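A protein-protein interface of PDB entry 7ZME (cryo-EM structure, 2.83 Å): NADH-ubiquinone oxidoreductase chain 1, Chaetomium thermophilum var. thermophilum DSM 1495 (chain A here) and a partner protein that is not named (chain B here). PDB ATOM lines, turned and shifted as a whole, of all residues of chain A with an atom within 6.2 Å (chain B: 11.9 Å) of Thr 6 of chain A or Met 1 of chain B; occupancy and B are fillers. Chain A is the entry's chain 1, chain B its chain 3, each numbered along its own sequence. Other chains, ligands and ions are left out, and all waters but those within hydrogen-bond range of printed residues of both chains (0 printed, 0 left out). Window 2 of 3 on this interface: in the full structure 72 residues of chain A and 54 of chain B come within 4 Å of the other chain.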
ATOM      1  N   SER A   4      10.838  20.345  -6.273  1.00  0.00           N
ATOM      2  CA  SER A   4      11.808  19.647  -5.440  1.00  0.00           C
ATOM      3  C   SER A   4      13.131  19.453  -6.171  1.00  0.00           C
ATOM      4  O   SER A   4      13.177  19.260  -7.387  1.00  0.00           O
ATOM      5  CB  SER A   4      11.252  18.290  -5.009  1.00  0.00           C
ATOM      6  OG  SER A   4      12.279  17.453  -4.516  1.00  0.00           O
ATOM      7  N   GLN A   5      14.221  19.512  -5.404  1.00  0.00           N
ATOM      8  CA  GLN A   5      15.548  19.305  -5.972  1.00  0.00           C
ATOM      9  C   GLN A   5      15.770  17.846  -6.345  1.00  0.00           C
ATOM     10  O   GLN A   5      16.348  17.550  -7.396  1.00  0.00           O
ATOM     11  CB  GLN A   5      16.615  19.776  -4.986  1.00  0.00           C
ATOM     12  CG  GLN A   5      18.031  19.378  -5.351  1.00  0.00           C
ATOM     13  CD  GLN A   5      18.706  20.386  -6.257  1.00  0.00           C
ATOM     14  OE1 GLN A   5      18.806  21.567  -5.926  1.00  0.00           O
ATOM     15  NE2 GLN A   5      19.182  19.923  -7.407  1.00  0.00           N
ATOM     16  N   THR A   6      15.325  16.920  -5.495  1.00  0.00           N
ATOM     17  CA  THR A   6      15.524  15.503  -5.777  1.00  0.00           C
ATOM     18  C   THR A   6      14.745  15.070  -7.012  1.00  0.00           C
ATOM     19  O   THR A   6      15.232  14.260  -7.809  1.00  0.00           O
ATOM     20  CB  THR A   6      15.121  14.665  -4.565  1.00  0.00           C
ATOM     21  OG1 THR A   6      15.927  15.037  -3.441  1.00  0.00           O
ATOM     22  CG2 THR A   6      15.323  13.188  -4.845  1.00  0.00           C
ATOM     23  N   ILE A   7      13.537  15.608  -7.192  1.00  0.00           N
ATOM     24  CA  ILE A   7      12.742  15.266  -8.364  1.00  0.00           C
ATOM     25  C   ILE A   7      13.384  15.823  -9.626  1.00  0.00           C
ATOM     26  O   ILE A   7      13.353  15.187 -10.686  1.00  0.00           O
ATOM     27  CB  ILE A   7      11.298  15.762  -8.188  1.00  0.00           C
ATOM     28  CG1 ILE A   7      10.679  15.130  -6.943  1.00  0.00           C
ATOM     29  CG2 ILE A   7      10.465  15.428  -9.409  1.00  0.00           C
ATOM     30  CD1 ILE A   7      10.603  13.622  -7.006  1.00  0.00           C
ATOM     31  N   ASN A   8      13.971  17.017  -9.540  1.00  0.00           N
ATOM     32  CA  ASN A   8      14.673  17.571 -10.691  1.00  0.00           C
ATOM     33  C   ASN A   8      15.823  16.669 -11.106  1.00  0.00           C
ATOM     34  O   ASN A   8      15.920  16.262 -12.268  1.00  0.00           O
ATOM     35  CB  ASN A   8      15.182  18.977 -10.374  1.00  0.00           C
ATOM     36  CG  ASN A   8      15.897  19.615 -11.547  1.00  0.00           C
ATOM     37  OD1 ASN A   8      17.110  19.814 -11.518  1.00  0.00           O
ATOM     38  ND2 ASN A   8      15.145  19.941 -12.588  1.00  0.00           N
ATOM     39  N   SER A   9      16.685  16.315 -10.154  1.00  0.00           N
ATOM     40  CA  SER A   9      17.828  15.459 -10.448  1.00  0.00           C
ATOM     41  C   SER A   9      17.389  14.078 -10.906  1.00  0.00           C
ATOM     42  O   SER A   9      18.058  13.458 -11.739  1.00  0.00           O
ATOM     43  CB  SER A   9      18.714  15.351  -9.212  1.00  0.00           C
ATOM     44  OG  SER A   9      18.969  16.632  -8.668  1.00  0.00           O
ATOM     45  N   LEU A  10      16.283  13.577 -10.359  1.00  0.00           N
ATOM     46  CA  LEU A  10      15.712  12.324 -10.834  1.00  0.00           C
ATOM     47  C   LEU A  10      15.376  12.408 -12.316  1.00  0.00           C
ATOM     48  O   LEU A  10      15.763  11.540 -13.104  1.00  0.00           O
ATOM     49  CB  LEU A  10      14.464  11.990 -10.017  1.00  0.00           C
ATOM     50  CG  LEU A  10      13.745  10.676 -10.312  1.00  0.00           C
ATOM     51  CD1 LEU A  10      14.657   9.507 -10.017  1.00  0.00           C
ATOM     52  CD2 LEU A  10      12.459  10.573  -9.510  1.00  0.00           C
ATOM     53  N   VAL A  11      14.649  13.444 -12.730  1.00  0.00           N
ATOM     54  CA  VAL A  11      14.192  13.543 -14.148  1.00  0.00           C
ATOM     55  C   VAL A  11      15.397  13.830 -15.042  1.00  0.00           C
ATOM     56  O   VAL A  11      15.453  13.278 -16.136  1.00  0.00           O
ATOM     57  CB  VAL A  11      13.090  14.606 -14.291  1.00  0.00           C
ATOM     58  CG1 VAL A  11      12.735  14.885 -15.742  1.00  0.00           C
ATOM     59  CG2 VAL A  11      11.846  14.216 -13.514  1.00  0.00           C
ATOM     60  N   MET B   1      18.432  16.151  -3.669  1.00  0.00           N
ATOM     61  CA  MET B   1      19.675  15.421  -3.889  1.00  0.00           C
ATOM     62  C   MET B   1      20.252  15.773  -5.255  1.00  0.00           C
ATOM     63  O   MET B   1      19.510  16.081  -6.185  1.00  0.00           O
ATOM     64  CB  MET B   1      19.438  13.915  -3.768  1.00  0.00           C
ATOM     65  CG  MET B   1      20.690  13.068  -3.857  1.00  0.00           C
ATOM     66  SD  MET B   1      20.346  11.306  -3.692  1.00  0.00           S
ATOM     67  CE  MET B   1      19.945  11.204  -1.949  1.00  0.00           C
ATOM     68  N   SER B   2      21.576  15.735  -5.363  1.00  0.00           N
ATOM     69  CA  SER B   2      22.253  16.153  -6.581  1.00  0.00           C
ATOM     70  C   SER B   2      22.061  15.135  -7.698  1.00  0.00           C
ATOM     71  O   SER B   2      21.887  13.938  -7.460  1.00  0.00           O
ATOM     72  CB  SER B   2      23.743  16.346  -6.323  1.00  0.00           C
ATOM     73  OG  SER B   2      24.365  15.109  -6.030  1.00  0.00           O
ATOM     74  N   ALA B   3      22.108  15.632  -8.934  1.00  0.00           N
ATOM     75  CA  ALA B   3      21.999  14.755 -10.094  1.00  0.00           C
ATOM     76  C   ALA B   3      23.163  13.779 -10.160  1.00  0.00           C
ATOM     77  O   ALA B   3      22.984  12.615 -10.537  1.00  0.00           O
ATOM     78  CB  ALA B   3      21.921  15.587 -11.373  1.00  0.00           C
ATOM     79  N   MET B   4      24.363  14.235  -9.805  1.00  0.00           N
ATOM     80  CA  MET B   4      25.541  13.382  -9.892  1.00  0.00           C
ATOM     81  C   MET B   4      25.405  12.159  -8.994  1.00  0.00           C
ATOM     82  O   MET B   4      25.682  11.031  -9.415  1.00  0.00           O
ATOM     83  CB  MET B   4      26.787  14.186  -9.527  1.00  0.00           C
ATOM     84  CG  MET B   4      28.076  13.407  -9.635  1.00  0.00           C
ATOM     85  SD  MET B   4      28.600  13.184 -11.340  1.00  0.00           S
ATOM     86  CE  MET B   4      28.831  11.411 -11.369  1.00  0.00           C
ATOM     87  N   SER B   5      24.976  12.366  -7.749  1.00  0.00           N
ATOM     88  CA  SER B   5      24.813  11.246  -6.830  1.00  0.00           C
ATOM     89  C   SER B   5      23.705  10.309  -7.290  1.00  0.00           C
ATOM     90  O   SER B   5      23.849   9.085  -7.213  1.00  0.00           O
ATOM     91  CB  SER B   5      24.530  11.764  -5.425  1.00  0.00           C
ATOM     92  OG  SER B   5      23.459  12.686  -5.437  1.00  0.00           O
ATOM     93  N   ILE B   6      22.594  10.869  -7.770  1.00  0.00           N
ATOM     94  CA  ILE B   6      21.499  10.049  -8.277  1.00  0.00           C
ATOM     95  C   ILE B   6      21.935   9.283  -9.519  1.00  0.00           C
ATOM     96  O   ILE B   6      21.523   8.136  -9.735  1.00  0.00           O
ATOM     97  CB  ILE B   6      20.263  10.929  -8.538  1.00  0.00           C
ATOM     98  CG1 ILE B   6      19.628  11.349  -7.213  1.00  0.00           C
ATOM     99  CG2 ILE B   6      19.253  10.218  -9.415  1.00  0.00           C
ATOM    100  CD1 ILE B   6      18.434  12.255  -7.362  1.00  0.00           C
ATOM    101  N   TYR B   7      22.773   9.898 -10.356  1.00  0.00           N
ATOM    102  CA  TYR B   7      23.281   9.205 -11.534  1.00  0.00           C
ATOM    103  C   TYR B   7      24.074   7.966 -11.141  1.00  0.00           C
ATOM    104  O   TYR B   7      23.899   6.896 -11.732  1.00  0.00           O
ATOM    105  CB  TYR B   7      24.140  10.160 -12.365  1.00  0.00           C
ATOM    106  CG  TYR B   7      24.498   9.662 -13.748  1.00  0.00           C
ATOM    107  CD1 TYR B   7      25.562   8.796 -13.940  1.00  0.00           C
ATOM    108  CD2 TYR B   7      23.783  10.075 -14.863  1.00  0.00           C
ATOM    109  CE1 TYR B   7      25.899   8.347 -15.194  1.00  0.00           C
ATOM    110  CE2 TYR B   7      24.114   9.631 -16.122  1.00  0.00           C
ATOM    111  CZ  TYR B   7      25.174   8.765 -16.282  1.00  0.00           C
ATOM    112  OH  TYR B   7      25.518   8.309 -17.531  1.00  0.00           O
ATOM    113  N   ILE B   8      24.944   8.090 -10.136  1.00  0.00           N
ATOM    114  CA  ILE B   8      25.698   6.936  -9.656  1.00  0.00           C
ATOM    115  C   ILE B   8      24.755   5.874  -9.106  1.00  0.00           C
ATOM    116  O   ILE B   8      24.993   4.671  -9.261  1.00  0.00           O
ATOM    117  CB  ILE B   8      26.735   7.372  -8.605  1.00  0.00           C
ATOM    118  CG1 ILE B   8      27.607   8.505  -9.145  1.00  0.00           C
ATOM    119  CG2 ILE B   8      27.603   6.196  -8.193  1.00  0.00           C
ATOM    120  CD1 ILE B   8      28.514   9.122  -8.110  1.00  0.00           C
ATOM    121  N   ILE B   9      23.675   6.301  -8.450  1.00  0.00           N
ATOM    122  CA  ILE B   9      22.711   5.346  -7.909  1.00  0.00           C
ATOM    123  C   ILE B   9      22.093   4.520  -9.028  1.00  0.00           C
ATOM    124  O   ILE B   9      22.063   3.288  -8.963  1.00  0.00           O
ATOM    125  CB  ILE B   9      21.634   6.072  -7.082  1.00  0.00           C
ATOM    126  CG1 ILE B   9      22.261   6.738  -5.860  1.00  0.00           C
ATOM    127  CG2 ILE B   9      20.537   5.106  -6.662  1.00  0.00           C
ATOM    128  CD1 ILE B   9      22.882   5.763  -4.890  1.00  0.00           C
ATOM    129  N   PHE B  10      21.604   5.180 -10.079  1.00  0.00           N
ATOM    130  CA  PHE B  10      20.937   4.458 -11.160  1.00  0.00           C
ATOM    131  C   PHE B  10      21.872   3.485 -11.862  1.00  0.00           C
ATOM    132  O   PHE B  10      21.535   2.310 -12.029  1.00  0.00           O
ATOM    133  CB  PHE B  10      20.319   5.429 -12.165  1.00  0.00           C
ATOM    134  CG  PHE B  10      18.956   5.907 -11.778  1.00  0.00           C
ATOM    135  CD1 PHE B  10      17.850   5.110 -12.020  1.00  0.00           C
ATOM    136  CD2 PHE B  10      18.773   7.128 -11.166  1.00  0.00           C
ATOM    137  CE1 PHE B  10      16.585   5.526 -11.669  1.00  0.00           C
ATOM    138  CE2 PHE B  10      17.506   7.551 -10.811  1.00  0.00           C
ATOM    139  CZ  PHE B  10      16.413   6.747 -11.062  1.00  0.00           C
ATOM    140  N   VAL B  11      23.055   3.942 -12.273  1.00  0.00           N
ATOM    141  CA  VAL B  11      23.928   3.053 -13.034  1.00  0.00           C
ATOM    142  C   VAL B  11      24.267   1.813 -12.219  1.00  0.00           C
ATOM    143  O   VAL B  11      24.467   0.726 -12.775  1.00  0.00           O
ATOM    144  CB  VAL B  11      25.196   3.792 -13.500  1.00  0.00           C
ATOM    145  CG1 VAL B  11      24.848   4.813 -14.567  1.00  0.00           C
ATOM    146  CG2 VAL B  11      25.901   4.445 -12.332  1.00  0.00           C
ATOM    147  N   ILE B  13      22.132   0.414  -9.923  1.00  0.00           N
ATOM    148  CA  ILE B  13      20.946  -0.431  -9.897  1.00  0.00           C
ATOM    149  C   ILE B  13      20.639  -1.036 -11.263  1.00  0.00           C
ATOM    150  O   ILE B  13      19.975  -2.075 -11.331  1.00  0.00           O
ATOM    151  CB  ILE B  13      19.732   0.344  -9.345  1.00  0.00           C
ATOM    152  CG1 ILE B  13      19.192   1.337 -10.371  1.00  0.00           C
ATOM    153  CG2 ILE B  13      20.089   1.041  -8.047  1.00  0.00           C
ATOM    154  CD1 ILE B  13      17.943   2.054  -9.923  1.00  0.00           C
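No residue of chain B comes within 4 Å of Ser 4 of chain A. Of chain B, only Met 1 (3.7 Å) comes within 4 Å of Gln 5 of chain A. Printed residues of chain B within 4 Å of Thr 6 of chain A: Met 1 (2.8 Å) and Ile 6 (3.8 Å). No residue of chain B comes within 4 Å of Ile 7 of chain A. Asn 8 of chain A touches none of the printed residues of chain B. Of chain B, only Met 1 (2.6 Å), Ser 2 (3.6 Å), Ala 3 (3.3 Å) and Ile 6 (3.6 Å) come within 4 Å of Ser 9 of chain A. Printed residues of chain B within 4 Å of Leu 10 of chain A: Ile 6 and Phe 10. Met 1 of chain B touches three residues of chain A. Of the printed residues of chain A, Ser 2 of chain B touches Ser 9. Of the printed residues of chain A, Ala 3 of chain B touches Ser 9. Of the printed residues of chain A, Ile 6 of chain B touches Thr 6 (3.8 Å), Ser 9 (3.6 Å) and Leu 10 (3.9 Å). Of the printed residues of chain A, Phe 10 of chain B touches Leu 10. The nearest residue of chain A that does not touch Met 1 of chain B is Leu 10 of chain A (5.8 Å). The nearest printed residue of chain A that does not touch Ser 2 of chain B is Gln 5 of chain A (4.9 Å).
Of the 12 printed residues of chain B, 5 touch a printed residue of chain A. Hydrophobic or aromatic side chains of chain B that line the printed part of chain A: Met 1, Ala 3, Ile 6 and Phe 10. Printed residues of chain A that touch a printed residue of chain B: Gln 5, Thr 6, Ser 9 and Leu 10. Hydrophobic or aromatic side chains of chain A within 4 Å of the printed part of chain B: Leu 10. Among the printed residues, 9 pairs touch across the chains.
The backbone NH (N) of Met 1 of chain B sits at hydrogen-bond distance from the side-chain hydroxyl (OG1) of Thr 6 of chain A. OG of Ser 9 of chain A is in hydrogen-bond range of O of Met 1 of chain B (2.6 Å). The side-chain hydroxyl of Ser 9 of chain A lies within hydrogen-bond range of the backbone NH of Ala 3 of chain B.
Among the printed residues, merely in contact across the chains: Gln 5 of chain A with Met 1 of chain B, Thr 6 of chain A with Ile 6 of chain B, Ser 9 of chain A with Ser 2 of chain B, Ser 9 of chain A with Ile 6 of chain B, Leu 10 of chain A with Ile 6 of chain B and Leu 10 of chain A with Phe 10 of chain B.
The side-chain hydroxyl (OG) of Ser 4 of chain A lies within hydrogen-bond range of the backbone NH (N) of Thr 6 of chain A. OG of Ser 9 of chain A sits at hydrogen-bond distance from O of Gln 5 of chain A (3.1 Å). OG of Ser 2 of chain B lies within hydrogen-bond range of OG of Ser 5 of chain B, 2.7 Å away.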
